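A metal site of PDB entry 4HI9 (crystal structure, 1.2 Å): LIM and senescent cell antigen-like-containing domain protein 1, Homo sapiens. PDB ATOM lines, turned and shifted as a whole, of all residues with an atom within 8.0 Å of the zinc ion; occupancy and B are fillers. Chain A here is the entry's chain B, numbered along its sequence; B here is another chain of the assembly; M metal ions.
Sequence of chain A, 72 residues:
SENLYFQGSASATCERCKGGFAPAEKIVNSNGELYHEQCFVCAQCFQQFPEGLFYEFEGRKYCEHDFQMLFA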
ATOM      1  N   VAL A  41     -14.739 -12.437  21.734  1.00  0.00           N
ATOM      2  CA  VAL A  41     -14.771 -11.131  22.352  1.00  0.00           C
ATOM      3  C   VAL A  41     -13.324 -10.709  22.576  1.00  0.00           C
ATOM      4  O   VAL A  41     -12.419 -11.537  22.579  1.00  0.00           O
ATOM      5  CB  VAL A  41     -15.522 -11.113  23.715  1.00  0.00           C
ATOM      6  CG1 VAL A  41     -16.997 -11.529  23.530  1.00  0.00           C
ATOM      7  CG2 VAL A  41     -14.832 -12.003  24.751  1.00  0.00           C
ATOM      8  N   CYS A  42     -13.121  -9.424  22.805  1.00  0.00           N
ATOM      9  CA  CYS A  42     -11.788  -8.926  23.102  1.00  0.00           C
ATOM     10  C   CYS A  42     -11.265  -9.480  24.430  1.00  0.00           C
ATOM     11  O   CYS A  42     -11.978  -9.491  25.445  1.00  0.00           O
ATOM     12  CB  CYS A  42     -11.848  -7.401  23.151  1.00  0.00           C
ATOM     13  SG  CYS A  42     -10.312  -6.599  23.689  1.00  0.00           S
ATOM     14  N   ALA A  43     -10.004  -9.893  24.420  1.00  0.00           N
ATOM     15  CA  ALA A  43      -9.390 -10.454  25.611  1.00  0.00           C
ATOM     16  C   ALA A  43      -9.187  -9.436  26.731  1.00  0.00           C
ATOM     17  O   ALA A  43      -9.041  -9.820  27.895  1.00  0.00           O
ATOM     18  CB  ALA A  43      -8.028 -11.061  25.271  1.00  0.00           C
ATOM     19  N   GLN A  44      -9.164  -8.155  26.383  1.00  0.00           N
ATOM     20  CA  GLN A  44      -8.962  -7.109  27.395  1.00  0.00           C
ATOM     21  C   GLN A  44     -10.260  -6.562  28.003  1.00  0.00           C
ATOM     22  O   GLN A  44     -10.352  -6.398  29.233  1.00  0.00           O
ATOM     23  CB  GLN A  44      -8.126  -5.974  26.815  1.00  0.00           C
ATOM     24  CG  GLN A  44      -7.667  -4.962  27.859  1.00  0.00           C
ATOM     25  CD  GLN A  44      -6.585  -5.537  28.757  1.00  0.00           C
ATOM     26  OE1 GLN A  44      -6.066  -6.625  28.488  1.00  0.00           O
ATOM     27  NE2 GLN A  44      -6.242  -4.838  29.825  1.00  0.00           N
ATOM     28  N   CYS A  45     -11.277  -6.285  27.183  1.00  0.00           N
ATOM     29  CA  CYS A  45     -12.518  -5.709  27.654  1.00  0.00           C
ATOM     30  C   CYS A  45     -13.676  -6.725  27.761  1.00  0.00           C
ATOM     31  O   CYS A  45     -14.682  -6.407  28.385  1.00  0.00           O
ATOM     32  CB  CYS A  45     -12.946  -4.492  26.807  1.00  0.00           C
ATOM     33  SG  CYS A  45     -13.298  -4.884  25.077  1.00  0.00           S
ATOM     34  N   PHE A  46     -13.509  -7.902  27.141  1.00  0.00           N
ATOM     35  CA  PHE A  46     -14.509  -8.967  27.095  1.00  0.00           C
ATOM     36  C   PHE A  46     -15.766  -8.586  26.322  1.00  0.00           C
ATOM     37  O   PHE A  46     -16.781  -9.281  26.437  1.00  0.00           O
ATOM     38  CB  PHE A  46     -14.937  -9.479  28.505  1.00  0.00           C
ATOM     39  CG  PHE A  46     -13.800  -9.608  29.507  1.00  0.00           C
ATOM     40  CD1 PHE A  46     -12.623 -10.264  29.200  1.00  0.00           C
ATOM     41  CD2 PHE A  46     -13.986  -9.102  30.792  1.00  0.00           C
ATOM     42  CE1 PHE A  46     -11.608 -10.352  30.180  1.00  0.00           C
ATOM     43  CE2 PHE A  46     -12.994  -9.212  31.759  1.00  0.00           C
ATOM     44  CZ  PHE A  46     -11.816  -9.851  31.465  1.00  0.00           C
ATOM     45  N   GLN A  47     -15.682  -7.555  25.487  1.00  0.00           N
ATOM     46  CA  GLN A  47     -16.833  -7.107  24.731  1.00  0.00           C
ATOM     47  C   GLN A  47     -16.673  -7.516  23.276  1.00  0.00           C
ATOM     48  O   GLN A  47     -15.598  -7.802  22.802  1.00  0.00           O
ATOM     49  CB  GLN A  47     -17.000  -5.589  24.877  1.00  0.00           C
ATOM     50  CG  GLN A  47     -17.378  -5.141  26.313  1.00  0.00           C
ATOM     51  CD  GLN A  47     -18.782  -5.556  26.719  1.00  0.00           C
ATOM     52  OE1 GLN A  47     -19.709  -5.390  25.945  1.00  0.00           O
ATOM     53  NE2 GLN A  47     -18.940  -6.083  27.933  1.00  0.00           N
ATOM     54  N   GLN A  48     -17.797  -7.595  22.584  1.00  0.00           N
ATOM     55  CA  GLN A  48     -17.755  -7.936  21.162  1.00  0.00           C
ATOM     56  C   GLN A  48     -16.888  -6.969  20.367  1.00  0.00           C
ATOM     57  O   GLN A  48     -16.754  -5.792  20.706  1.00  0.00           O
ATOM     58  CB  GLN A  48     -19.172  -8.023  20.607  1.00  0.00           C
ATOM     59  CG  GLN A  48     -19.730  -9.401  20.763  1.00  0.00           C
ATOM     60  CD  GLN A  48     -19.873  -9.848  22.186  1.00  0.00           C
ATOM     61  OE1 GLN A  48     -19.628  -9.100  23.127  1.00  0.00           O
ATOM     62  NE2 GLN A  48     -20.260 -11.099  22.358  1.00  0.00           N
ATOM     63  N   PHE A  49     -16.286  -7.465  19.299  1.00  0.00           N
ATOM     64  CA  PHE A  49     -15.474  -6.623  18.431  1.00  0.00           C
ATOM     65  C   PHE A  49     -16.347  -5.714  17.586  1.00  0.00           C
ATOM     66  O   PHE A  49     -17.192  -6.222  16.858  1.00  0.00           O
ATOM     67  CB  PHE A  49     -14.638  -7.491  17.499  1.00  0.00           C
ATOM     68  CG  PHE A  49     -13.739  -8.453  18.215  1.00  0.00           C
ATOM     69  CD1 PHE A  49     -12.688  -7.990  18.964  1.00  0.00           C
ATOM     70  CD2 PHE A  49     -13.937  -9.825  18.115  1.00  0.00           C
ATOM     71  CE1 PHE A  49     -11.848  -8.866  19.605  1.00  0.00           C
ATOM     72  CE2 PHE A  49     -13.099 -10.704  18.769  1.00  0.00           C
ATOM     73  CZ  PHE A  49     -12.033 -10.208  19.525  1.00  0.00           C
ATOM     74  N   PRO A  50     -16.144  -4.394  17.657  1.00  0.00           N
ATOM     75  CA  PRO A  50     -16.920  -3.539  16.747  1.00  0.00           C
ATOM     76  C   PRO A  50     -16.755  -3.977  15.286  1.00  0.00           C
ATOM     77  O   PRO A  50     -15.629  -4.059  14.784  1.00  0.00           O
ATOM     78  CB  PRO A  50     -16.322  -2.154  16.992  1.00  0.00           C
ATOM     79  CG  PRO A  50     -15.868  -2.184  18.402  1.00  0.00           C
ATOM     80  CD  PRO A  50     -15.327  -3.586  18.583  1.00  0.00           C
ATOM     81  N   LYS A  61      -6.827 -12.163  21.043  1.00  0.00           N
ATOM     82  CA  LYS A  61      -7.493 -11.246  20.120  1.00  0.00           C
ATOM     83  C   LYS A  61      -8.027 -10.024  20.841  1.00  0.00           C
ATOM     84  O   LYS A  61      -8.625 -10.175  21.910  1.00  0.00           O
ATOM     85  CB  LYS A  61      -8.663 -11.974  19.461  1.00  0.00           C
ATOM     86  CG  LYS A  61      -8.212 -13.150  18.593  1.00  0.00           C
ATOM     87  CD  LYS A  61      -9.390 -13.817  17.888  1.00  0.00           C
ATOM     88  CE  LYS A  61      -8.899 -14.884  16.894  1.00  0.00           C
ATOM     89  NZ  LYS A  61      -8.252 -16.051  17.597  1.00  0.00           N
ATOM     90  N   TYR A  62      -7.812  -8.856  20.264  1.00  0.00           N
ATOM     91  CA  TYR A  62      -8.148  -7.583  20.895  1.00  0.00           C
ATOM     92  C   TYR A  62      -8.940  -6.697  19.944  1.00  0.00           C
ATOM     93  O   TYR A  62      -8.713  -6.707  18.734  1.00  0.00           O
ATOM     94  CB  TYR A  62      -6.868  -6.830  21.311  1.00  0.00           C
ATOM     95  CG  TYR A  62      -6.052  -7.624  22.294  1.00  0.00           C
ATOM     96  CD1 TYR A  62      -6.285  -7.520  23.681  1.00  0.00           C
ATOM     97  CD2 TYR A  62      -5.079  -8.525  21.862  1.00  0.00           C
ATOM     98  CE1 TYR A  62      -5.570  -8.270  24.596  1.00  0.00           C
ATOM     99  CE2 TYR A  62      -4.360  -9.294  22.788  1.00  0.00           C
ATOM    100  CZ  TYR A  62      -4.611  -9.154  24.142  1.00  0.00           C
ATOM    101  OH  TYR A  62      -3.867  -9.915  25.008  1.00  0.00           O
ATOM    102  N   CYS A  63      -9.821  -5.880  20.500  1.00  0.00           N
ATOM    103  CA  CYS A  63     -10.448  -4.828  19.725  1.00  0.00           C
ATOM    104  C   CYS A  63      -9.429  -3.746  19.362  1.00  0.00           C
ATOM    105  O   CYS A  63      -8.340  -3.660  19.932  1.00  0.00           O
ATOM    106  CB  CYS A  63     -11.650  -4.247  20.460  1.00  0.00           C
ATOM    107  SG  CYS A  63     -11.200  -3.244  21.977  1.00  0.00           S
ATOM    108  N   GLU A  64      -9.823  -2.894  18.421  1.00  0.00           N
ATOM    109  CA  GLU A  64      -8.941  -1.818  18.003  1.00  0.00           C
ATOM    110  C   GLU A  64      -8.512  -0.923  19.166  1.00  0.00           C
ATOM    111  O   GLU A  64      -7.312  -0.570  19.302  1.00  0.00           O
ATOM    112  CB  GLU A  64      -9.618  -0.972  16.913  1.00  0.00           C
ATOM    113  CG  GLU A  64      -8.701   0.104  16.338  1.00  0.00           C
ATOM    114  CD  GLU A  64      -9.294   0.789  15.127  1.00  0.00           C
ATOM    115  OE1 GLU A  64     -10.447   0.461  14.752  1.00  0.00           O
ATOM    116  OE2 GLU A  64      -8.613   1.647  14.546  1.00  0.00           O
ATOM    117  N   HIS A  65      -9.477  -0.544  20.001  1.00  0.00           N
ATOM    118  CA  HIS A  65      -9.175   0.342  21.110  1.00  0.00           C
ATOM    119  C   HIS A  65      -8.098  -0.254  22.009  1.00  0.00           C
ATOM    120  O   HIS A  65      -7.097   0.405  22.313  1.00  0.00           O
ATOM    121  CB  HIS A  65     -10.431   0.630  21.945  1.00  0.00           C
ATOM    122  CG  HIS A  65     -10.151   1.380  23.208  1.00  0.00           C
ATOM    123  ND1 HIS A  65      -9.938   2.739  23.224  1.00  0.00           N
ATOM    124  CD2 HIS A  65     -10.007   0.947  24.479  1.00  0.00           C
ATOM    125  CE1 HIS A  65      -9.671   3.117  24.462  1.00  0.00           C
ATOM    126  NE2 HIS A  65      -9.685   2.056  25.238  1.00  0.00           N
ATOM    127  N   ASP A  66      -8.304  -1.498  22.468  1.00  0.00           N
ATOM    128  CA  ASP A  66      -7.338  -2.084  23.408  1.00  0.00           C
ATOM    129  C   ASP A  66      -6.006  -2.396  22.731  1.00  0.00           C
ATOM    130  O   ASP A  66      -4.939  -2.305  23.365  1.00  0.00           O
ATOM    131  CB  ASP A  66      -7.969  -3.310  24.058  1.00  0.00           C
ATOM    132  CG  ASP A  66      -9.000  -2.930  25.103  1.00  0.00           C
ATOM    133  OD1 ASP A  66      -8.665  -2.020  25.894  1.00  0.00           O
ATOM    134  OD2 ASP A  66     -10.126  -3.458  25.128  1.00  0.00           O
ATOM    135  N   PHE A  67      -6.031  -2.800  21.462  1.00  0.00           N
ATOM    136  CA  PHE A  67      -4.810  -3.084  20.702  1.00  0.00           C
ATOM    137  C   PHE A  67      -3.961  -1.793  20.610  1.00  0.00           C
ATOM    138  O   PHE A  67      -2.739  -1.802  20.856  1.00  0.00           O
ATOM    139  CB  PHE A  67      -5.077  -3.659  19.310  1.00  0.00           C
ATOM    140  CG  PHE A  67      -3.850  -4.063  18.594  1.00  0.00           C
ATOM    141  CD1 PHE A  67      -3.225  -5.259  18.887  1.00  0.00           C
ATOM    142  CD2 PHE A  67      -3.283  -3.232  17.640  1.00  0.00           C
ATOM    143  CE1 PHE A  67      -2.063  -5.635  18.206  1.00  0.00           C
ATOM    144  CE2 PHE A  67      -2.134  -3.604  16.979  1.00  0.00           C
ATOM    145  CZ  PHE A  67      -1.522  -4.806  17.275  1.00  0.00           C
ATOM    146  N   LEU A  70      -2.463  -0.812  24.139  1.00  0.00           N
ATOM    147  CA  LEU A  70      -1.495  -1.688  24.769  1.00  0.00           C
ATOM    148  C   LEU A  70      -0.355  -2.193  23.917  1.00  0.00           C
ATOM    149  O   LEU A  70       0.722  -2.420  24.464  1.00  0.00           O
ATOM    150  CB  LEU A  70      -2.226  -2.921  25.344  1.00  0.00           C
ATOM    151  CG  LEU A  70      -3.267  -2.602  26.423  1.00  0.00           C
ATOM    152  CD1 LEU A  70      -4.038  -3.853  26.822  1.00  0.00           C
ATOM    153  CD2 LEU A  70      -2.574  -1.980  27.634  1.00  0.00           C
ATOM    154  N   GLU B 103      -8.798   0.280  33.045  1.00  0.00           N
ATOM    155  CA  GLU B 103      -9.655   1.264  32.400  1.00  0.00           C
ATOM    156  C   GLU B 103     -11.067   0.752  32.114  1.00  0.00           C
ATOM    157  O   GLU B 103     -11.971   1.561  31.893  1.00  0.00           O
ATOM    158  CB  GLU B 103      -9.021   1.777  31.101  1.00  0.00           C
ATOM    159  CG  GLU B 103      -9.037   0.817  29.944  1.00  0.00           C
ATOM    160  CD  GLU B 103      -8.823   1.519  28.604  1.00  0.00           C
ATOM    161  OE1 GLU B 103      -9.744   2.207  28.093  1.00  0.00           O
ATOM    162  OE2 GLU B 103      -7.719   1.381  28.050  1.00  0.00           O
ATOM    163  N   HIS B 104     -11.239  -0.566  32.091  1.00  0.00           N
ATOM    164  CA  HIS B 104     -12.516  -1.182  31.851  1.00  0.00           C
ATOM    165  C   HIS B 104     -13.223  -1.555  33.147  1.00  0.00           C
ATOM    166  O   HIS B 104     -14.325  -2.121  33.115  1.00  0.00           O
ATOM    167  CB  HIS B 104     -12.390  -2.423  30.966  1.00  0.00           C
ATOM    168  CG  HIS B 104     -11.829  -2.101  29.616  1.00  0.00           C
ATOM    169  ND1 HIS B 104     -12.522  -1.352  28.692  1.00  0.00           N
ATOM    170  CD2 HIS B 104     -10.607  -2.357  29.069  1.00  0.00           C
ATOM    171  CE1 HIS B 104     -11.762  -1.186  27.618  1.00  0.00           C
ATOM    172  NE2 HIS B 104     -10.597  -1.769  27.831  1.00  0.00           N
ATOM    173  N   TYR B 137     -18.984  -2.487  32.455  1.00  0.00           N
ATOM    174  CA  TYR B 137     -20.009  -2.992  31.549  1.00  0.00           C
ATOM    175  C   TYR B 137     -20.911  -3.970  32.300  1.00  0.00           C
ATOM    176  O   TYR B 137     -21.665  -4.722  31.681  1.00  0.00           O
ATOM    177  CB  TYR B 137     -19.343  -3.646  30.310  1.00  0.00           C
ATOM    178  CG  TYR B 137     -18.212  -2.777  29.789  1.00  0.00           C
ATOM    179  CD1 TYR B 137     -18.429  -1.457  29.432  1.00  0.00           C
ATOM    180  CD2 TYR B 137     -16.919  -3.261  29.753  1.00  0.00           C
ATOM    181  CE1 TYR B 137     -17.392  -0.635  29.054  1.00  0.00           C
ATOM    182  CE2 TYR B 137     -15.860  -2.458  29.354  1.00  0.00           C
ATOM    183  CZ  TYR B 137     -16.092  -1.130  29.025  1.00  0.00           C
ATOM    184  OH  TYR B 137     -15.046  -0.283  28.680  1.00  0.00           O
HETATM  185 ZN    ZN M   1     -11.283  -4.499  23.989  1.00  0.00          ZN
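Of the 21 residues printed, 4 come within 4 Å of the zinc ion.
Along chain A the residues within 4 Å of the zinc ion span positions 42 to 66.
The zinc ion is bound by OD2 of Asp 66, SG of Cys 45, SG of Cys 42 and SG of Cys 63.
The zinc ion has four donor atoms within binding distance.
The side-chain carboxylate (OD1) of Asp 66 sits at hydrogen-bond distance from a ring nitrogen (NE2) of His 104 of chain B (2.7 Å).
SG of Cys 45 lies close to N of Gln 47, at 3.6 Å.
The backbone NH (N) of Gln 44 sits close to the side-chain sulfur (SG) of Cys 42, at 3.3 Å.
N of Cys 42 lies within hydrogen-bond range of O of Gln 47.
SG of Cys 63 lies close to N of His 65 (3.8 Å).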
